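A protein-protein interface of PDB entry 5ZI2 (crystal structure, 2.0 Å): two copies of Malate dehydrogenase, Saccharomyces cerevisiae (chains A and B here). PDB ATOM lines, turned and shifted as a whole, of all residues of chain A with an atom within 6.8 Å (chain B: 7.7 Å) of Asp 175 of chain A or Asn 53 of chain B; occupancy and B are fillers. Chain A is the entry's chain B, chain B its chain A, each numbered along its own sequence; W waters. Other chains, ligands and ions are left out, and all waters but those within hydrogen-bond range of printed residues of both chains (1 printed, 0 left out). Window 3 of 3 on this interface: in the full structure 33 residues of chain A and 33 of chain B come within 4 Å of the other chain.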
ATOM      1  N   GLU A 156      -0.231 -17.009  36.094  1.00  0.00           N
ATOM      2  CA  GLU A 156       0.105 -16.961  34.673  1.00  0.00           C
ATOM      3  C   GLU A 156      -0.695 -15.894  33.884  1.00  0.00           C
ATOM      4  O   GLU A 156      -0.139 -15.167  33.063  1.00  0.00           O
ATOM      5  CB  GLU A 156      -0.151 -18.345  34.055  1.00  0.00           C
ATOM      6  CG  GLU A 156       0.796 -19.418  34.562  1.00  0.00           C
ATOM      7  CD  GLU A 156       0.543 -20.767  33.871  1.00  0.00           C
ATOM      8  OE1 GLU A 156       1.126 -21.003  32.791  1.00  0.00           O
ATOM      9  OE2 GLU A 156      -0.320 -21.543  34.371  1.00  0.00           O
ATOM     10  N   VAL A 160       0.813 -11.764  32.811  1.00  0.00           N
ATOM     11  CA  VAL A 160       0.715 -11.205  31.490  1.00  0.00           C
ATOM     12  C   VAL A 160      -0.133  -9.924  31.517  1.00  0.00           C
ATOM     13  O   VAL A 160       0.265  -8.919  30.905  1.00  0.00           O
ATOM     14  CB  VAL A 160       0.238 -12.225  30.422  1.00  0.00           C
ATOM     15  CG1 VAL A 160      -0.032 -11.529  29.082  1.00  0.00           C
ATOM     16  CG2 VAL A 160       1.252 -13.334  30.245  1.00  0.00           C
ATOM     17  N   GLY A 171       4.847  -7.430  27.426  1.00  0.00           N
ATOM     18  CA  GLY A 171       3.554  -8.085  27.607  1.00  0.00           C
ATOM     19  C   GLY A 171       3.061  -8.816  26.362  1.00  0.00           C
ATOM     20  O   GLY A 171       2.689 -10.009  26.421  1.00  0.00           O
ATOM     21  N   GLN A 172       3.086  -8.093  25.238  1.00  0.00           N
ATOM     22  CA  GLN A 172       2.733  -8.628  23.887  1.00  0.00           C
ATOM     23  C   GLN A 172       3.578  -9.858  23.547  1.00  0.00           C
ATOM     24  O   GLN A 172       3.136 -10.743  22.839  1.00  0.00           O
ATOM     25  CB  GLN A 172       2.892  -7.524  22.779  1.00  0.00           C
ATOM     26  CG  GLN A 172       1.842  -6.382  22.814  1.00  0.00           C
ATOM     27  CD  GLN A 172       2.246  -5.037  22.125  1.00  0.00           C
ATOM     28  OE1 GLN A 172       3.328  -4.879  21.511  1.00  0.00           O
ATOM     29  NE2 GLN A 172       1.341  -4.055  22.225  1.00  0.00           N
ATOM     30  N   GLU A 173       4.796  -9.919  24.065  1.00  0.00           N
ATOM     31  CA  GLU A 173       5.656 -11.084  23.833  1.00  0.00           C
ATOM     32  C   GLU A 173       5.265 -12.391  24.582  1.00  0.00           C
ATOM     33  O   GLU A 173       5.870 -13.432  24.294  1.00  0.00           O
ATOM     34  CB  GLU A 173       7.127 -10.738  24.178  1.00  0.00           C
ATOM     35  CG  GLU A 173       8.040 -10.436  22.994  1.00  0.00           C
ATOM     36  CD  GLU A 173       9.495 -10.310  23.434  1.00  0.00           C
ATOM     37  OE1 GLU A 173      10.386 -10.777  22.688  1.00  0.00           O
ATOM     38  OE2 GLU A 173       9.746  -9.775  24.543  1.00  0.00           O
ATOM     39  N   GLN A 174       4.339 -12.343  25.558  1.00  0.00           N
ATOM     40  CA  GLN A 174       4.115 -13.481  26.443  1.00  0.00           C
ATOM     41  C   GLN A 174       2.931 -14.332  25.974  1.00  0.00           C
ATOM     42  O   GLN A 174       1.996 -13.839  25.390  1.00  0.00           O
ATOM     43  CB  GLN A 174       3.840 -13.018  27.870  1.00  0.00           C
ATOM     44  CG  GLN A 174       4.834 -12.028  28.462  1.00  0.00           C
ATOM     45  CD  GLN A 174       6.261 -12.543  28.492  1.00  0.00           C
ATOM     46  OE1 GLN A 174       6.525 -13.662  28.890  1.00  0.00           O
ATOM     47  NE2 GLN A 174       7.183 -11.727  28.064  1.00  0.00           N
ATOM     48  N   ASP A 175       2.981 -15.609  26.259  1.00  0.00           N
ATOM     49  CA  ASP A 175       1.896 -16.499  25.983  1.00  0.00           C
ATOM     50  C   ASP A 175       1.326 -16.938  27.351  1.00  0.00           C
ATOM     51  O   ASP A 175       2.016 -17.588  28.158  1.00  0.00           O
ATOM     52  CB  ASP A 175       2.455 -17.624  25.098  1.00  0.00           C
ATOM     53  CG  ASP A 175       1.421 -18.634  24.700  1.00  0.00           C
ATOM     54  OD1 ASP A 175       0.312 -18.676  25.328  1.00  0.00           O
ATOM     55  OD2 ASP A 175       1.726 -19.441  23.800  1.00  0.00           O
ATOM     56  N   LYS A 176       0.079 -16.562  27.653  1.00  0.00           N
ATOM     57  CA  LYS A 176      -0.508 -16.979  28.933  1.00  0.00           C
ATOM     58  C   LYS A 176      -0.458 -18.490  29.194  1.00  0.00           C
ATOM     59  O   LYS A 176      -0.355 -18.893  30.329  1.00  0.00           O
ATOM     60  CB  LYS A 176      -1.934 -16.535  29.052  1.00  0.00           C
ATOM     61  CG  LYS A 176      -2.074 -15.143  29.545  1.00  0.00           C
ATOM     62  CD  LYS A 176      -3.516 -14.683  29.471  1.00  0.00           C
ATOM     63  CE  LYS A 176      -3.575 -13.208  29.818  1.00  0.00           C
ATOM     64  NZ  LYS A 176      -4.939 -12.626  29.687  1.00  0.00           N
ATOM     65  N   THR A 177      -0.526 -19.305  28.152  1.00  0.00           N
ATOM     66  CA  THR A 177      -0.530 -20.760  28.290  1.00  0.00           C
ATOM     67  C   THR A 177       0.861 -21.354  28.705  1.00  0.00           C
ATOM     68  O   THR A 177       0.903 -22.476  29.176  1.00  0.00           O
ATOM     69  CB  THR A 177      -1.037 -21.438  27.016  1.00  0.00           C
ATOM     70  OG1 THR A 177      -0.060 -21.354  25.980  1.00  0.00           O
ATOM     71  CG2 THR A 177      -2.447 -20.832  26.530  1.00  0.00           C
ATOM     72  N   THR A 178       1.971 -20.603  28.536  1.00  0.00           N
ATOM     73  CA  THR A 178       3.330 -21.089  28.873  1.00  0.00           C
ATOM     74  C   THR A 178       4.007 -20.311  30.000  1.00  0.00           C
ATOM     75  O   THR A 178       5.215 -20.508  30.264  1.00  0.00           O
ATOM     76  CB  THR A 178       4.273 -21.065  27.620  1.00  0.00           C
ATOM     77  OG1 THR A 178       4.299 -19.767  27.047  1.00  0.00           O
ATOM     78  CG2 THR A 178       3.736 -21.990  26.561  1.00  0.00           C
ATOM     79  N   MET A 179       3.243 -19.478  30.709  1.00  0.00           N
ATOM     80  CA  MET A 179       3.803 -18.653  31.790  1.00  0.00           C
ATOM     81  C   MET A 179       4.280 -19.461  33.020  1.00  0.00           C
ATOM     82  O   MET A 179       5.027 -18.933  33.849  1.00  0.00           O
ATOM     83  CB  MET A 179       2.794 -17.572  32.228  1.00  0.00           C
ATOM     84  CG  MET A 179       2.624 -16.445  31.248  1.00  0.00           C
ATOM     85  SD  MET A 179       4.160 -15.604  30.751  1.00  0.00           S
ATOM     86  CE  MET A 179       4.792 -15.015  32.292  1.00  0.00           C
ATOM     87  N   HIS A 180       3.855 -20.714  33.149  1.00  0.00           N
ATOM     88  CA  HIS A 180       4.357 -21.582  34.190  1.00  0.00           C
ATOM     89  C   HIS A 180       5.909 -21.761  34.141  1.00  0.00           C
ATOM     90  O   HIS A 180       6.536 -22.066  35.156  1.00  0.00           O
ATOM     91  CB  HIS A 180       3.620 -22.905  34.147  1.00  0.00           C
ATOM     92  CG  HIS A 180       3.588 -23.536  32.802  1.00  0.00           C
ATOM     93  ND1 HIS A 180       4.650 -24.268  32.306  1.00  0.00           N
ATOM     94  CD2 HIS A 180       2.631 -23.550  31.829  1.00  0.00           C
ATOM     95  CE1 HIS A 180       4.343 -24.723  31.102  1.00  0.00           C
ATOM     96  NE2 HIS A 180       3.128 -24.307  30.794  1.00  0.00           N
ATOM     97  N   MET B   3      -6.621 -12.564  14.753  1.00  0.00           N
ATOM     98  CA  MET B   3      -7.492 -13.461  15.599  1.00  0.00           C
ATOM     99  C   MET B   3      -8.840 -12.817  15.740  1.00  0.00           C
ATOM    100  O   MET B   3      -8.914 -11.614  15.532  1.00  0.00           O
ATOM    101  CB  MET B   3      -6.873 -13.698  16.962  1.00  0.00           C
ATOM    102  CG  MET B   3      -5.768 -14.750  17.020  1.00  0.00           C
ATOM    103  SD  MET B   3      -5.499 -15.323  18.720  1.00  0.00           S
ATOM    104  CE  MET B   3      -4.911 -13.872  19.621  1.00  0.00           C
ATOM    105  N   LYS B  24     -13.634 -19.598  25.704  1.00  0.00           N
ATOM    106  CA  LYS B  24     -12.463 -19.039  26.338  1.00  0.00           C
ATOM    107  C   LYS B  24     -11.174 -19.849  26.042  1.00  0.00           C
ATOM    108  O   LYS B  24     -10.135 -19.267  25.940  1.00  0.00           O
ATOM    109  CB  LYS B  24     -12.669 -18.885  27.839  1.00  0.00           C
ATOM    110  CG  LYS B  24     -11.478 -18.267  28.620  1.00  0.00           C
ATOM    111  CD  LYS B  24     -11.347 -16.774  28.298  1.00  0.00           C
ATOM    112  CE  LYS B  24     -10.151 -16.110  28.987  1.00  0.00           C
ATOM    113  NZ  LYS B  24      -8.851 -16.205  28.254  1.00  0.00           N
ATOM    114  N   LEU B  25     -11.283 -21.172  25.874  1.00  0.00           N
ATOM    115  CA  LEU B  25     -10.156 -22.028  25.671  1.00  0.00           C
ATOM    116  C   LEU B  25      -9.696 -22.006  24.228  1.00  0.00           C
ATOM    117  O   LEU B  25      -8.608 -22.475  23.978  1.00  0.00           O
ATOM    118  CB  LEU B  25     -10.498 -23.475  26.080  1.00  0.00           C
ATOM    119  CG  LEU B  25     -11.116 -23.734  27.453  1.00  0.00           C
ATOM    120  CD1 LEU B  25     -11.018 -25.161  27.855  1.00  0.00           C
ATOM    121  CD2 LEU B  25     -10.436 -22.925  28.522  1.00  0.00           C
ATOM    122  N   SER B  26     -10.445 -21.383  23.299  1.00  0.00           N
ATOM    123  CA  SER B  26     -10.088 -21.465  21.895  1.00  0.00           C
ATOM    124  C   SER B  26      -8.880 -20.616  21.533  1.00  0.00           C
ATOM    125  O   SER B  26      -8.888 -19.456  21.795  1.00  0.00           O
ATOM    126  CB  SER B  26     -11.224 -21.020  21.009  1.00  0.00           C
ATOM    127  OG  SER B  26     -10.810 -20.950  19.662  1.00  0.00           O
ATOM    128  N   PRO B  27      -7.904 -21.182  20.798  1.00  0.00           N
ATOM    129  CA  PRO B  27      -6.764 -20.378  20.352  1.00  0.00           C
ATOM    130  C   PRO B  27      -7.084 -19.449  19.189  1.00  0.00           C
ATOM    131  O   PRO B  27      -6.247 -18.637  18.808  1.00  0.00           O
ATOM    132  CB  PRO B  27      -5.706 -21.452  19.916  1.00  0.00           C
ATOM    133  CG  PRO B  27      -6.464 -22.706  19.703  1.00  0.00           C
ATOM    134  CD  PRO B  27      -7.706 -22.635  20.597  1.00  0.00           C
ATOM    135  N   VAL B  29      -9.644 -17.258  19.206  1.00  0.00           N
ATOM    136  CA  VAL B  29     -10.379 -16.137  19.706  1.00  0.00           C
ATOM    137  C   VAL B  29      -9.447 -15.117  20.333  1.00  0.00           C
ATOM    138  O   VAL B  29      -8.712 -15.439  21.297  1.00  0.00           O
ATOM    139  CB  VAL B  29     -11.379 -16.611  20.808  1.00  0.00           C
ATOM    140  CG1 VAL B  29     -12.107 -15.424  21.407  1.00  0.00           C
ATOM    141  CG2 VAL B  29     -12.403 -17.549  20.219  1.00  0.00           C
ATOM    142  N   SER B  30      -9.543 -13.875  19.902  1.00  0.00           N
ATOM    143  CA  SER B  30      -8.769 -12.762  20.516  1.00  0.00           C
ATOM    144  C   SER B  30      -9.500 -12.084  21.649  1.00  0.00           C
ATOM    145  O   SER B  30      -8.906 -11.794  22.635  1.00  0.00           O
ATOM    146  CB  SER B  30      -8.455 -11.673  19.478  1.00  0.00           C
ATOM    147  OG  SER B  30      -9.596 -11.449  18.671  1.00  0.00           O
ATOM    148  N   GLU B  31     -10.782 -11.786  21.470  1.00  0.00           N
ATOM    149  CA  GLU B  31     -11.640 -11.210  22.508  1.00  0.00           C
ATOM    150  C   GLU B  31     -12.955 -11.974  22.549  1.00  0.00           C
ATOM    151  O   GLU B  31     -13.539 -12.275  21.513  1.00  0.00           O
ATOM    152  CB  GLU B  31     -12.013  -9.756  22.171  1.00  0.00           C
ATOM    153  CG  GLU B  31     -10.869  -8.766  21.935  1.00  0.00           C
ATOM    154  CD  GLU B  31     -11.347  -7.497  21.220  1.00  0.00           C
ATOM    155  OE1 GLU B  31     -10.981  -7.297  20.033  1.00  0.00           O
ATOM    156  OE2 GLU B  31     -12.150  -6.752  21.820  1.00  0.00           O
ATOM    157  N   ILE B  50      -8.712 -17.465  33.537  1.00  0.00           N
ATOM    158  CA  ILE B  50      -8.165 -18.628  32.794  1.00  0.00           C
ATOM    159  C   ILE B  50      -7.004 -18.187  31.938  1.00  0.00           C
ATOM    160  O   ILE B  50      -7.142 -17.264  31.174  1.00  0.00           O
ATOM    161  CB  ILE B  50      -9.229 -19.292  31.909  1.00  0.00           C
ATOM    162  CG1 ILE B  50     -10.307 -19.933  32.808  1.00  0.00           C
ATOM    163  CG2 ILE B  50      -8.640 -20.306  30.934  1.00  0.00           C
ATOM    164  CD1 ILE B  50     -11.449 -20.543  32.078  1.00  0.00           C
ATOM    165  N   ASN B  51      -5.923 -18.943  31.950  1.00  0.00           N
ATOM    166  CA  ASN B  51      -4.705 -18.558  31.200  1.00  0.00           C
ATOM    167  C   ASN B  51      -4.607 -19.007  29.779  1.00  0.00           C
ATOM    168  O   ASN B  51      -3.631 -19.709  29.359  1.00  0.00           O
ATOM    169  CB  ASN B  51      -3.439 -18.958  31.997  1.00  0.00           C
ATOM    170  CG  ASN B  51      -3.228 -20.478  32.074  1.00  0.00           C
ATOM    171  OD1 ASN B  51      -4.154 -21.229  32.370  1.00  0.00           O
ATOM    172  ND2 ASN B  51      -1.986 -20.931  31.829  1.00  0.00           N
ATOM    173  N   THR B  52      -5.556 -18.525  28.993  1.00  0.00           N
ATOM    174  CA  THR B  52      -5.479 -18.649  27.532  1.00  0.00           C
ATOM    175  C   THR B  52      -5.527 -17.185  27.018  1.00  0.00           C
ATOM    176  O   THR B  52      -5.913 -16.282  27.765  1.00  0.00           O
ATOM    177  CB  THR B  52      -6.698 -19.394  26.954  1.00  0.00           C
ATOM    178  OG1 THR B  52      -7.897 -18.795  27.480  1.00  0.00           O
ATOM    179  CG2 THR B  52      -6.630 -20.827  27.380  1.00  0.00           C
ATOM    180  N   ASN B  53      -5.097 -16.959  25.776  1.00  0.00           N
ATOM    181  CA  ASN B  53      -4.752 -15.626  25.380  1.00  0.00           C
ATOM    182  C   ASN B  53      -5.985 -14.677  25.131  1.00  0.00           C
ATOM    183  O   ASN B  53      -5.904 -13.475  25.322  1.00  0.00           O
ATOM    184  CB  ASN B  53      -3.689 -15.710  24.274  1.00  0.00           C
ATOM    185  CG  ASN B  53      -2.345 -16.206  24.845  1.00  0.00           C
ATOM    186  OD1 ASN B  53      -1.825 -15.616  25.794  1.00  0.00           O
ATOM    187  ND2 ASN B  53      -1.902 -17.359  24.410  1.00  0.00           N
ATOM    188  N   SER B  54      -7.163 -15.192  24.886  1.00  0.00           N
ATOM    189  CA  SER B  54      -8.296 -14.244  24.672  1.00  0.00           C
ATOM    190  C   SER B  54      -8.558 -13.258  25.845  1.00  0.00           C
ATOM    191  O   SER B  54      -8.396 -13.617  26.999  1.00  0.00           O
ATOM    192  CB  SER B  54      -9.515 -15.065  24.414  1.00  0.00           C
ATOM    193  OG  SER B  54      -9.722 -15.942  25.468  1.00  0.00           O
ATOM    194  N   SER B  55      -8.962 -12.026  25.589  1.00  0.00           N
ATOM    195  CA  SER B  55      -9.445 -11.195  26.695  1.00  0.00           C
ATOM    196  C   SER B  55     -10.959 -11.516  26.786  1.00  0.00           C
ATOM    197  O   SER B  55     -11.577 -11.720  25.776  1.00  0.00           O
ATOM    198  CB  SER B  55      -9.199  -9.708  26.459  1.00  0.00           C
ATOM    199  OG  SER B  55     -10.131  -9.269  25.499  1.00  0.00           O
ATOM    200  N   CYS B  56     -11.517 -11.593  27.984  1.00  0.00           N
ATOM    201  CA  CYS B  56     -12.882 -11.991  28.176  1.00  0.00           C
ATOM    202  C   CYS B  56     -13.521 -11.007  29.111  1.00  0.00           C
ATOM    203  O   CYS B  56     -13.058 -10.875  30.248  1.00  0.00           O
ATOM    204  CB  CYS B  56     -12.956 -13.388  28.836  1.00  0.00           C
ATOM    205  SG  CYS B  56     -14.669 -13.931  29.094  1.00  0.00           S
HETATM  206  O   HOH W   1      -7.307 -14.613  30.536  1.00  0.00           O
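Of the printed residues of chain B, Glu 156 of chain A touches Asn 51 (3.1 Å).
Printed residues of chain B within 4 Å of Asp 175 of chain A: Asn 53 (2.7 Å).
Printed residues of chain B within 4 Å of Lys 176 of chain A: Asn 51, Thr 52 and Asn 53.
The nearest residue of chain B that does not touch Asp 175 of chain A is Asn 51 of chain B (5.7 Å).
ND2 of Asn 51 of chain B sits at hydrogen-bond distance from OE2 of Glu 156 of chain A.
ND2 of Asn 51 of chain B is in hydrogen-bond range of O of Lys 176 of chain A (3.0 Å).
N of Thr 177 of chain A sits close to O of Asn 51 of chain B (3.4 Å).
The side-chain carboxylate of Asp 175 of chain A sits at hydrogen-bond distance from the side-chain amide nitrogen of Asn 53 of chain B (2.7 Å).
The side-chain amide oxygen (OD1) of Asn 53 of chain B sits at hydrogen-bond distance from the backbone NH (N) of Lys 176 of chain A.
The backbone carbonyl oxygen of Lys 24 of chain B lies within hydrogen-bond range of the side-chain hydroxyl of Thr 52 of chain B.
The side-chain carboxylate (OE1) of Glu 156 of chain A is in hydrogen-bond range of the backbone NH (N) of Met 179 of chain A (3.3 Å).
The side-chain carboxylate (OE1) of Glu 156 of chain A is in hydrogen-bond range of the backbone NH (N) of His 180 of chain A, 2.8 Å away.
OG1 of Thr 177 of chain A lies within hydrogen-bond range of OD1 of Asp 175 of chain A (2.8 Å).
The backbone carbonyl oxygen (O) of Asp 175 of chain A sits at hydrogen-bond distance from the side-chain hydroxyl (OG1) of Thr 178 of chain A, 3.3 Å away.
The backbone carbonyl oxygen of Thr 177 of chain A lies within hydrogen-bond range of a ring nitrogen (NE2) of His 180 of chain A (3.3 Å).
Among the printed residues, merely in contact across the chains: Lys 176 of chain A with Thr 52 of chain B (3.3 Å) and Thr 177 of chain A with Thr 52 of chain B (3.9 Å).
Of the 12 printed residues of chain A, 4 touch a printed residue of chain B.
Printed residues of chain A that touch a printed residue of chain B: Glu 156, Asp 175, Lys 176 and Thr 177.
Along chain A the printed residues that touch a printed residue of chain B span positions 156 to 177.
No position is printed for both chains.
Of the 7 pairs that touch across the chains among the printed residues, none has its exchanged pair printed and touching as well.
Water W1 lies within hydrogen-bond range of the backbone carbonyl oxygen of Ile 50 of chain B (2.7 Å), the side-chain amino group of Lys 24 of chain B (3.2 Å) and the side-chain amino group of Lys 176 of chain A (3.2 Å).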
